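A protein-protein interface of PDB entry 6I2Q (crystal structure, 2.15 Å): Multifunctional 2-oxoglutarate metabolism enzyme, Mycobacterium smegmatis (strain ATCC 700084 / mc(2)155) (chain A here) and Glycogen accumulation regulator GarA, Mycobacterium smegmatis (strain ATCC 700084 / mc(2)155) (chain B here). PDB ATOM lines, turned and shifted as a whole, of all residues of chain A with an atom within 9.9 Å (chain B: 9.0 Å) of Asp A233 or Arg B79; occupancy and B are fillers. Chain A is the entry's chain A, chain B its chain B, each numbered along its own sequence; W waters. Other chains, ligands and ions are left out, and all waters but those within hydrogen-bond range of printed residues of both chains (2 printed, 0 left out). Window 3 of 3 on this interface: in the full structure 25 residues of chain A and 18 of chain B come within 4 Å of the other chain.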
ATOM      1  N   ALA A 118     -34.092  27.015  11.829  1.00  0.00           N
ATOM      2  CA  ALA A 118     -34.086  25.553  11.802  1.00  0.00           C
ATOM      3  C   ALA A 118     -34.887  24.970  12.969  1.00  0.00           C
ATOM      4  O   ALA A 118     -35.621  24.003  12.771  1.00  0.00           O
ATOM      5  CB  ALA A 118     -32.661  25.025  11.815  1.00  0.00           C
ATOM      6  N   ASP A 164     -35.924  15.472  23.901  1.00  0.00           N
ATOM      7  CA  ASP A 164     -34.693  16.058  23.361  1.00  0.00           C
ATOM      8  C   ASP A 164     -33.810  16.652  24.494  1.00  0.00           C
ATOM      9  O   ASP A 164     -32.592  16.448  24.492  1.00  0.00           O
ATOM     10  CB  ASP A 164     -34.998  17.144  22.322  1.00  0.00           C
ATOM     11  CG  ASP A 164     -33.712  17.697  21.721  1.00  0.00           C
ATOM     12  OD1 ASP A 164     -33.102  16.999  20.912  1.00  0.00           O
ATOM     13  OD2 ASP A 164     -33.314  18.813  22.096  1.00  0.00           O
ATOM     14  N   ALA A 167     -32.149  13.920  26.351  1.00  0.00           N
ATOM     15  CA  ALA A 167     -31.047  13.433  25.521  1.00  0.00           C
ATOM     16  C   ALA A 167     -29.869  14.414  25.575  1.00  0.00           C
ATOM     17  O   ALA A 167     -28.724  13.970  25.630  1.00  0.00           O
ATOM     18  CB  ALA A 167     -31.510  13.219  24.083  1.00  0.00           C
ATOM     19  N   GLU A 168     -30.142  15.731  25.637  1.00  0.00           N
ATOM     20  CA  GLU A 168     -29.096  16.757  25.753  1.00  0.00           C
ATOM     21  C   GLU A 168     -28.303  16.573  27.086  1.00  0.00           C
ATOM     22  O   GLU A 168     -27.111  16.870  27.129  1.00  0.00           O
ATOM     23  CB  GLU A 168     -29.722  18.166  25.662  1.00  0.00           C
ATOM     24  CG  GLU A 168     -28.741  19.295  25.384  1.00  0.00           C
ATOM     25  CD  GLU A 168     -28.061  19.367  24.025  1.00  0.00           C
ATOM     26  OE1 GLU A 168     -28.453  18.631  23.092  1.00  0.00           O
ATOM     27  OE2 GLU A 168     -27.115  20.173  23.903  1.00  0.00           O
ATOM     28  N   HIS A 169     -28.963  16.040  28.144  1.00  0.00           N
ATOM     29  CA  HIS A 169     -28.326  15.753  29.440  1.00  0.00           C
ATOM     30  C   HIS A 169     -27.690  14.363  29.441  1.00  0.00           C
ATOM     31  O   HIS A 169     -27.118  13.957  30.452  1.00  0.00           O
ATOM     32  CB  HIS A 169     -29.338  15.872  30.597  1.00  0.00           C
ATOM     33  CG  HIS A 169     -29.685  17.281  30.960  1.00  0.00           C
ATOM     34  ND1 HIS A 169     -28.987  17.966  31.939  1.00  0.00           N
ATOM     35  CD2 HIS A 169     -30.671  18.076  30.486  1.00  0.00           C
ATOM     36  CE1 HIS A 169     -29.577  19.143  32.043  1.00  0.00           C
ATOM     37  NE2 HIS A 169     -30.585  19.262  31.175  1.00  0.00           N
ATOM     38  N   GLY A 170     -27.797  13.652  28.314  1.00  0.00           N
ATOM     39  CA  GLY A 170     -27.215  12.322  28.119  1.00  0.00           C
ATOM     40  C   GLY A 170     -27.862  11.240  28.958  1.00  0.00           C
ATOM     41  O   GLY A 170     -27.214  10.270  29.338  1.00  0.00           O
ATOM     42  N   TYR A 227     -35.403   7.401  20.451  1.00  0.00           N
ATOM     43  CA  TYR A 227     -35.462   8.789  20.034  1.00  0.00           C
ATOM     44  C   TYR A 227     -34.042   9.252  19.640  1.00  0.00           C
ATOM     45  O   TYR A 227     -33.090   9.039  20.403  1.00  0.00           O
ATOM     46  CB  TYR A 227     -36.051   9.670  21.145  1.00  0.00           C
ATOM     47  CG  TYR A 227     -36.160  11.127  20.767  1.00  0.00           C
ATOM     48  CD1 TYR A 227     -37.362  11.660  20.297  1.00  0.00           C
ATOM     49  CD2 TYR A 227     -35.069  11.989  20.899  1.00  0.00           C
ATOM     50  CE1 TYR A 227     -37.465  13.004  19.940  1.00  0.00           C
ATOM     51  CE2 TYR A 227     -35.163  13.332  20.550  1.00  0.00           C
ATOM     52  CZ  TYR A 227     -36.361  13.835  20.068  1.00  0.00           C
ATOM     53  OH  TYR A 227     -36.451  15.168  19.750  1.00  0.00           O
ATOM     54  N   ILE A 228     -33.918   9.897  18.458  1.00  0.00           N
ATOM     55  CA  ILE A 228     -32.654  10.437  17.948  1.00  0.00           C
ATOM     56  C   ILE A 228     -32.747  11.959  17.944  1.00  0.00           C
ATOM     57  O   ILE A 228     -33.725  12.499  17.435  1.00  0.00           O
ATOM     58  CB  ILE A 228     -32.369   9.869  16.522  1.00  0.00           C
ATOM     59  CG1 ILE A 228     -32.252   8.326  16.543  1.00  0.00           C
ATOM     60  CG2 ILE A 228     -31.150  10.543  15.812  1.00  0.00           C
ATOM     61  CD1 ILE A 228     -32.401   7.702  15.141  1.00  0.00           C
ATOM     62  N   GLN A 229     -31.737  12.654  18.488  1.00  0.00           N
ATOM     63  CA  GLN A 229     -31.735  14.120  18.452  1.00  0.00           C
ATOM     64  C   GLN A 229     -31.555  14.631  17.037  1.00  0.00           C
ATOM     65  O   GLN A 229     -30.741  14.107  16.267  1.00  0.00           O
ATOM     66  CB  GLN A 229     -30.636  14.713  19.327  1.00  0.00           C
ATOM     67  CG  GLN A 229     -30.910  14.614  20.823  1.00  0.00           C
ATOM     68  CD  GLN A 229     -29.829  15.312  21.599  1.00  0.00           C
ATOM     69  OE1 GLN A 229     -28.696  14.846  21.659  1.00  0.00           O
ATOM     70  NE2 GLN A 229     -30.148  16.457  22.193  1.00  0.00           N
ATOM     71  N   MET A 230     -32.306  15.666  16.708  1.00  0.00           N
ATOM     72  CA  MET A 230     -32.255  16.325  15.412  1.00  0.00           C
ATOM     73  C   MET A 230     -31.010  17.221  15.311  1.00  0.00           C
ATOM     74  O   MET A 230     -30.360  17.251  14.271  1.00  0.00           O
ATOM     75  CB  MET A 230     -33.548  17.147  15.207  1.00  0.00           C
ATOM     76  CG  MET A 230     -33.574  17.944  13.932  1.00  0.00           C
ATOM     77  SD  MET A 230     -33.725  16.912  12.457  1.00  0.00           S
ATOM     78  CE  MET A 230     -33.203  18.107  11.215  1.00  0.00           C
ATOM     79  N   PHE A 231     -30.693  17.954  16.372  1.00  0.00           N
ATOM     80  CA  PHE A 231     -29.579  18.899  16.347  1.00  0.00           C
ATOM     81  C   PHE A 231     -28.417  18.496  17.266  1.00  0.00           C
ATOM     82  O   PHE A 231     -27.374  19.149  17.239  1.00  0.00           O
ATOM     83  CB  PHE A 231     -30.086  20.313  16.703  1.00  0.00           C
ATOM     84  CG  PHE A 231     -31.156  20.793  15.740  1.00  0.00           C
ATOM     85  CD1 PHE A 231     -32.483  20.897  16.145  1.00  0.00           C
ATOM     86  CD2 PHE A 231     -30.846  21.077  14.413  1.00  0.00           C
ATOM     87  CE1 PHE A 231     -33.473  21.318  15.252  1.00  0.00           C
ATOM     88  CE2 PHE A 231     -31.838  21.486  13.518  1.00  0.00           C
ATOM     89  CZ  PHE A 231     -33.144  21.610  13.944  1.00  0.00           C
ATOM     90  N   GLY A 232     -28.590  17.433  18.034  1.00  0.00           N
ATOM     91  CA  GLY A 232     -27.571  16.935  18.952  1.00  0.00           C
ATOM     92  C   GLY A 232     -27.021  15.598  18.511  1.00  0.00           C
ATOM     93  O   GLY A 232     -27.455  15.028  17.499  1.00  0.00           O
ATOM     94  N   ASP A 233     -26.077  15.077  19.294  1.00  0.00           N
ATOM     95  CA  ASP A 233     -25.344  13.840  18.990  1.00  0.00           C
ATOM     96  C   ASP A 233     -25.847  12.606  19.731  1.00  0.00           C
ATOM     97  O   ASP A 233     -25.318  11.520  19.519  1.00  0.00           O
ATOM     98  CB  ASP A 233     -23.860  14.072  19.336  1.00  0.00           C
ATOM     99  CG  ASP A 233     -23.269  15.247  18.579  1.00  0.00           C
ATOM    100  OD1 ASP A 233     -23.493  15.339  17.356  1.00  0.00           O
ATOM    101  OD2 ASP A 233     -22.612  16.084  19.211  1.00  0.00           O
ATOM    102  N   ASN A 234     -26.853  12.758  20.589  1.00  0.00           N
ATOM    103  CA  ASN A 234     -27.336  11.644  21.408  1.00  0.00           C
ATOM    104  C   ASN A 234     -28.657  11.054  20.948  1.00  0.00           C
ATOM    105  O   ASN A 234     -29.459  11.692  20.257  1.00  0.00           O
ATOM    106  CB  ASN A 234     -27.497  12.120  22.880  1.00  0.00           C
ATOM    107  CG  ASN A 234     -26.196  12.571  23.509  1.00  0.00           C
ATOM    108  OD1 ASN A 234     -25.124  12.158  23.099  1.00  0.00           O
ATOM    109  ND2 ASN A 234     -26.248  13.435  24.509  1.00  0.00           N
ATOM    110  N   ASP A 235     -28.872   9.820  21.403  1.00  0.00           N
ATOM    111  CA  ASP A 235     -30.068   9.010  21.309  1.00  0.00           C
ATOM    112  C   ASP A 235     -30.567   8.759  22.740  1.00  0.00           C
ATOM    113  O   ASP A 235     -29.777   8.793  23.688  1.00  0.00           O
ATOM    114  CB  ASP A 235     -29.765   7.672  20.620  1.00  0.00           C
ATOM    115  CG  ASP A 235     -29.448   7.716  19.131  1.00  0.00           C
ATOM    116  OD1 ASP A 235     -29.443   8.836  18.542  1.00  0.00           O
ATOM    117  OD2 ASP A 235     -29.215   6.639  18.551  1.00  0.00           O
ATOM    118  N   ILE A 236     -31.864   8.488  22.906  1.00  0.00           N
ATOM    119  CA  ILE A 236     -32.418   8.172  24.222  1.00  0.00           C
ATOM    120  C   ILE A 236     -33.539   7.192  23.989  1.00  0.00           C
ATOM    121  O   ILE A 236     -34.220   7.286  22.964  1.00  0.00           O
ATOM    122  CB  ILE A 236     -32.845   9.460  25.005  1.00  0.00           C
ATOM    123  CG1 ILE A 236     -33.132   9.152  26.502  1.00  0.00           C
ATOM    124  CG2 ILE A 236     -33.998  10.221  24.324  1.00  0.00           C
ATOM    125  CD1 ILE A 236     -33.083  10.318  27.454  1.00  0.00           C
ATOM    126  N   LYS B  17     -25.390   6.040   9.175  1.00  0.00           N
ATOM    127  CA  LYS B  17     -24.649   5.977  10.434  1.00  0.00           C
ATOM    128  C   LYS B  17     -25.565   6.257  11.627  1.00  0.00           C
ATOM    129  O   LYS B  17     -25.346   5.719  12.714  1.00  0.00           O
ATOM    130  CB  LYS B  17     -23.448   6.934  10.416  1.00  0.00           C
ATOM    131  CG  LYS B  17     -22.294   6.430   9.541  1.00  0.00           C
ATOM    132  CD  LYS B  17     -21.636   5.159  10.092  1.00  0.00           C
ATOM    133  CE  LYS B  17     -20.844   4.435   9.041  1.00  0.00           C
ATOM    134  NZ  LYS B  17     -20.239   3.190   9.575  1.00  0.00           N
ATOM    135  N   ARG B  18     -26.591   7.085  11.423  1.00  0.00           N
ATOM    136  CA  ARG B  18     -27.579   7.403  12.453  1.00  0.00           C
ATOM    137  C   ARG B  18     -28.943   7.412  11.812  1.00  0.00           C
ATOM    138  O   ARG B  18     -29.119   8.021  10.752  1.00  0.00           O
ATOM    139  CB  ARG B  18     -27.273   8.731  13.166  1.00  0.00           C
ATOM    140  CG  ARG B  18     -26.883   8.520  14.623  1.00  0.00           C
ATOM    141  CD  ARG B  18     -26.459   9.802  15.296  1.00  0.00           C
ATOM    142  NE  ARG B  18     -27.399  10.196  16.341  1.00  0.00           N
ATOM    143  CZ  ARG B  18     -27.582  11.447  16.743  1.00  0.00           C
ATOM    144  NH1 ARG B  18     -28.466  11.721  17.680  1.00  0.00           N
ATOM    145  NH2 ARG B  18     -26.884  12.434  16.203  1.00  0.00           N
ATOM    146  N   THR B  75     -31.047  20.259   4.451  1.00  0.00           N
ATOM    147  CA  THR B  75     -29.954  19.307   4.247  1.00  0.00           C
ATOM    148  C   THR B  75     -28.669  19.931   4.790  1.00  0.00           C
ATOM    149  O   THR B  75     -28.393  21.118   4.567  1.00  0.00           O
ATOM    150  CB  THR B  75     -29.830  18.906   2.754  1.00  0.00           C
ATOM    151  OG1 THR B  75     -31.119  18.580   2.230  1.00  0.00           O
ATOM    152  CG2 THR B  75     -28.891  17.721   2.534  1.00  0.00           C
ATOM    153  N   TYR B  76     -27.905  19.126   5.524  1.00  0.00           N
ATOM    154  CA  TYR B  76     -26.643  19.537   6.121  1.00  0.00           C
ATOM    155  C   TYR B  76     -25.503  18.702   5.572  1.00  0.00           C
ATOM    156  O   TYR B  76     -25.673  17.518   5.254  1.00  0.00           O
ATOM    157  CB  TYR B  76     -26.689  19.422   7.658  1.00  0.00           C
ATOM    158  CG  TYR B  76     -27.787  20.236   8.314  1.00  0.00           C
ATOM    159  CD1 TYR B  76     -27.506  21.443   8.945  1.00  0.00           C
ATOM    160  CD2 TYR B  76     -29.107  19.783   8.327  1.00  0.00           C
ATOM    161  CE1 TYR B  76     -28.514  22.196   9.549  1.00  0.00           C
ATOM    162  CE2 TYR B  76     -30.123  20.532   8.911  1.00  0.00           C
ATOM    163  CZ  TYR B  76     -29.821  21.732   9.534  1.00  0.00           C
ATOM    164  OH  TYR B  76     -30.827  22.464  10.110  1.00  0.00           O
ATOM    165  N   VAL B  77     -24.345  19.341   5.425  1.00  0.00           N
ATOM    166  CA  VAL B  77     -23.108  18.699   5.010  1.00  0.00           C
ATOM    167  C   VAL B  77     -22.103  19.078   6.072  1.00  0.00           C
ATOM    168  O   VAL B  77     -21.831  20.269   6.253  1.00  0.00           O
ATOM    169  CB  VAL B  77     -22.654  19.042   3.566  1.00  0.00           C
ATOM    170  CG1 VAL B  77     -21.341  18.334   3.218  1.00  0.00           C
ATOM    171  CG2 VAL B  77     -23.733  18.679   2.555  1.00  0.00           C
ATOM    172  N   ASN B  78     -21.620  18.072   6.832  1.00  0.00           N
ATOM    173  CA  ASN B  78     -20.675  18.221   7.946  1.00  0.00           C
ATOM    174  C   ASN B  78     -21.165  19.295   8.965  1.00  0.00           C
ATOM    175  O   ASN B  78     -20.419  20.220   9.311  1.00  0.00           O
ATOM    176  CB  ASN B  78     -19.252  18.532   7.413  1.00  0.00           C
ATOM    177  CG  ASN B  78     -18.669  17.395   6.611  1.00  0.00           C
ATOM    178  OD1 ASN B  78     -18.839  16.213   6.951  1.00  0.00           O
ATOM    179  ND2 ASN B  78     -17.970  17.727   5.524  1.00  0.00           N
ATOM    180  N   ARG B  79     -22.431  19.159   9.426  1.00  0.00           N
ATOM    181  CA  ARG B  79     -23.127  20.032  10.400  1.00  0.00           C
ATOM    182  C   ARG B  79     -23.405  21.454   9.850  1.00  0.00           C
ATOM    183  O   ARG B  79     -23.716  22.349  10.632  1.00  0.00           O
ATOM    184  CB  ARG B  79     -22.366  20.146  11.760  1.00  0.00           C
ATOM    185  CG  ARG B  79     -21.892  18.844  12.433  1.00  0.00           C
ATOM    186  CD  ARG B  79     -22.975  17.786  12.603  1.00  0.00           C
ATOM    187  NE  ARG B  79     -23.994  18.156  13.588  1.00  0.00           N
ATOM    188  CZ  ARG B  79     -23.932  17.855  14.882  1.00  0.00           C
ATOM    189  NH1 ARG B  79     -24.913  18.214  15.700  1.00  0.00           N
ATOM    190  NH2 ARG B  79     -22.887  17.196  15.369  1.00  0.00           N
ATOM    191  N   GLU B  80     -23.323  21.665   8.522  1.00  0.00           N
ATOM    192  CA  GLU B  80     -23.564  22.993   7.940  1.00  0.00           C
ATOM    193  C   GLU B  80     -24.734  22.961   6.950  1.00  0.00           C
ATOM    194  O   GLU B  80     -24.723  22.130   6.042  1.00  0.00           O
ATOM    195  CB  GLU B  80     -22.298  23.551   7.264  1.00  0.00           C
ATOM    196  CG  GLU B  80     -21.188  23.942   8.235  1.00  0.00           C
ATOM    197  CD  GLU B  80     -21.505  25.034   9.244  1.00  0.00           C
ATOM    198  OE1 GLU B  80     -22.186  26.020   8.877  1.00  0.00           O
ATOM    199  OE2 GLU B  80     -21.060  24.902  10.407  1.00  0.00           O
ATOM    200  N   PRO B  81     -25.749  23.851   7.107  1.00  0.00           N
ATOM    201  CA  PRO B  81     -26.890  23.840   6.173  1.00  0.00           C
ATOM    202  C   PRO B  81     -26.481  24.298   4.771  1.00  0.00           C
ATOM    203  O   PRO B  81     -25.675  25.216   4.636  1.00  0.00           O
ATOM    204  CB  PRO B  81     -27.883  24.808   6.827  1.00  0.00           C
ATOM    205  CG  PRO B  81     -27.019  25.757   7.597  1.00  0.00           C
ATOM    206  CD  PRO B  81     -25.905  24.907   8.132  1.00  0.00           C
ATOM    207  N   VAL B  82     -26.991  23.618   3.731  1.00  0.00           N
ATOM    208  CA  VAL B  82     -26.658  23.922   2.333  1.00  0.00           C
ATOM    209  C   VAL B  82     -27.884  23.781   1.414  1.00  0.00           C
ATOM    210  O   VAL B  82     -28.746  22.939   1.653  1.00  0.00           O
ATOM    211  CB  VAL B  82     -25.484  23.043   1.784  1.00  0.00           C
ATOM    212  CG1 VAL B  82     -24.171  23.281   2.536  1.00  0.00           C
ATOM    213  CG2 VAL B  82     -25.837  21.554   1.748  1.00  0.00           C
ATOM    214  N   ASP B  91     -17.562  12.719   3.890  1.00  0.00           N
ATOM    215  CA  ASP B  91     -18.522  13.761   4.289  1.00  0.00           C
ATOM    216  C   ASP B  91     -19.773  13.177   4.891  1.00  0.00           C
ATOM    217  O   ASP B  91     -20.233  12.113   4.468  1.00  0.00           O
ATOM    218  CB  ASP B  91     -18.924  14.654   3.106  1.00  0.00           C
ATOM    219  CG  ASP B  91     -17.947  15.764   2.771  1.00  0.00           C
ATOM    220  OD1 ASP B  91     -18.160  16.449   1.749  1.00  0.00           O
ATOM    221  OD2 ASP B  91     -16.971  15.950   3.534  1.00  0.00           O
ATOM    222  N   GLU B  92     -20.342  13.888   5.864  1.00  0.00           N
ATOM    223  CA  GLU B  92     -21.584  13.474   6.490  1.00  0.00           C
ATOM    224  C   GLU B  92     -22.741  14.357   6.003  1.00  0.00           C
ATOM    225  O   GLU B  92     -22.697  15.590   6.116  1.00  0.00           O
ATOM    226  CB  GLU B  92     -21.469  13.497   8.008  1.00  0.00           C
ATOM    227  CG  GLU B  92     -22.696  12.943   8.711  1.00  0.00           C
ATOM    228  CD  GLU B  92     -22.882  13.494  10.106  1.00  0.00           C
ATOM    229  OE1 GLU B  92     -22.718  12.719  11.073  1.00  0.00           O
ATOM    230  OE2 GLU B  92     -23.191  14.700  10.235  1.00  0.00           O
ATOM    231  N   VAL B  93     -23.765  13.701   5.446  1.00  0.00           N
ATOM    232  CA  VAL B  93     -24.999  14.304   4.942  1.00  0.00           C
ATOM    233  C   VAL B  93     -26.102  14.025   5.950  1.00  0.00           C
ATOM    234  O   VAL B  93     -26.339  12.860   6.275  1.00  0.00           O
ATOM    235  CB  VAL B  93     -25.388  13.766   3.539  1.00  0.00           C
ATOM    236  CG1 VAL B  93     -26.679  14.407   3.030  1.00  0.00           C
ATOM    237  CG2 VAL B  93     -24.250  13.950   2.534  1.00  0.00           C
ATOM    238  N   GLN B  94     -26.796  15.082   6.419  1.00  0.00           N
ATOM    239  CA  GLN B  94     -27.933  14.935   7.331  1.00  0.00           C
ATOM    240  C   GLN B  94     -29.226  15.265   6.582  1.00  0.00           C
ATOM    241  O   GLN B  94     -29.342  16.369   6.029  1.00  0.00           O
ATOM    242  CB  GLN B  94     -27.785  15.814   8.586  1.00  0.00           C
ATOM    243  CG  GLN B  94     -28.897  15.553   9.597  1.00  0.00           C
ATOM    244  CD  GLN B  94     -28.815  16.304  10.896  1.00  0.00           C
ATOM    245  OE1 GLN B  94     -27.771  16.852  11.265  1.00  0.00           O
ATOM    246  NE2 GLN B  94     -29.935  16.327  11.636  1.00  0.00           N
ATOM    247  N   ARG B  99     -28.313  10.447   9.397  1.00  0.00           N
ATOM    248  CA  ARG B  99     -26.922  10.834   9.123  1.00  0.00           C
ATOM    249  C   ARG B  99     -26.345   9.777   8.208  1.00  0.00           C
ATOM    250  O   ARG B  99     -26.342   8.592   8.555  1.00  0.00           O
ATOM    251  CB  ARG B  99     -26.072  11.000  10.408  1.00  0.00           C
ATOM    252  CG  ARG B  99     -26.168  12.374  11.092  1.00  0.00           C
ATOM    253  CD  ARG B  99     -27.440  12.538  11.903  1.00  0.00           C
ATOM    254  NE  ARG B  99     -27.333  13.624  12.879  1.00  0.00           N
ATOM    255  CZ  ARG B  99     -28.270  13.932  13.770  1.00  0.00           C
ATOM    256  NH1 ARG B  99     -29.404  13.232  13.826  1.00  0.00           N
ATOM    257  NH2 ARG B  99     -28.076  14.928  14.629  1.00  0.00           N
HETATM  258  O   HOH W   1     -27.462  18.478  13.535  1.00  0.00           O
HETATM  259  O   HOH W   2     -25.243  14.542  15.341  1.00  0.00           O
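Of chain B, only Arg B18 and Arg B79 come within 4 Å of Asp A233.
Of chain A, only Phe A231 and Asp A233 come within 4 Å of Arg B79.
Gly A232 touches two residues of chain B.
Asn A234 touches just one residue of chain B: Arg B18 (2.8 Å).
No residue of chain A comes within 4 Å of Glu B80.
Printed residues of chain B within 4 Å of Phe A231: Tyr B76 (3.7 Å) and Arg B79 (3.0 Å).
Printed residues of chain A within 4 Å of Gln B94: Met A230.
Of the printed residues of chain B, Asp A235 touches Arg B18 (3.2 Å).
Ile A236 touches none of the printed residues of chain B.
The nearest residue of chain B that does not touch Asp A233 is Arg B99 (5.1 Å).
The nearest residue of chain A that does not touch Arg B79 is Gly A232 (4.4 Å).
The nearest printed residue of chain B that does not touch Ala A118 is Pro B81 (6.9 Å).
The side-chain carboxylate of Asp A233 lies within salt-bridge range of the guanidinium group of Arg B79 (2.8 Å).
NH1 of Arg B18 is in hydrogen-bond range of O of Asn A234, at 2.8 Å.
O of Gly A232 sits at hydrogen-bond distance from NH2 of Arg B99.
The side-chain carboxylate of Asp A235 lies within salt-bridge range of the guanidinium group of Arg B18 (3.2 Å).
O of Gln A229 lies within hydrogen-bond range of NH1 of Arg B99.
O of Met A230 sits at hydrogen-bond distance from NE2 of Gln B94.
N of Gln A229 lies close to NH1 of Arg B18.
O of Gly A232 sits at hydrogen-bond distance from NH2 of Arg B18 (3.0 Å).
O of Met A230 lies within hydrogen-bond range of NH2 of Arg B99, 3.3 Å away.
The backbone carbonyl oxygen (O) of Phe A231 sits at hydrogen-bond distance from the guanidinium group (NH1) of Arg B79, 3.0 Å away.
O of Tyr B76 lies within hydrogen-bond range of N of Gln B94 (2.9 Å).
The side-chain carboxylate (OD1) of Asp A164 lies close to the side-chain amide nitrogen (NE2) of Gln A229 (3.3 Å).
The backbone carbonyl oxygen of Arg B18 sits at hydrogen-bond distance from the backbone NH of Arg B99, 2.9 Å away.
O of Ala A167 is in hydrogen-bond range of ND2 of Asn A234.
OE1 of Glu A168 sits at hydrogen-bond distance from NE2 of Gln A229, at 2.9 Å.
OE1 of Gln A229 sits at hydrogen-bond distance from N of Asn A234 (3.0 Å).
Of the 16 printed residues of chain A, 9 touch a printed residue of chain B.
Along chain A the printed residues that touch a printed residue of chain B span positions 118 to 235.
Hydrophobic or aromatic side chains of chain B that line the printed part of chain A: Tyr B76.
Water W2 lies within hydrogen-bond range of OD1 of Asp A233, NH2 of Arg B18, NH2 of Arg B99 and O of Gly A232.
Water W1 lies within hydrogen-bond range of the side-chain amide oxygen of Gln B94 (2.8 Å), the backbone carbonyl oxygen of Met A230 (3.2 Å) and the guanidinium group of Arg B79 (3.4 Å).
Among the printed residues, merely in contact across the chains: Asp A233 with Arg B18 (3.4 Å), Ile A228 with Arg B18 (3.5 Å), Ala A118 with Tyr B76 (3.6 Å), Phe A231 with Tyr B76 (3.7 Å) and Ile A228 with Arg B99 (3.8 Å).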
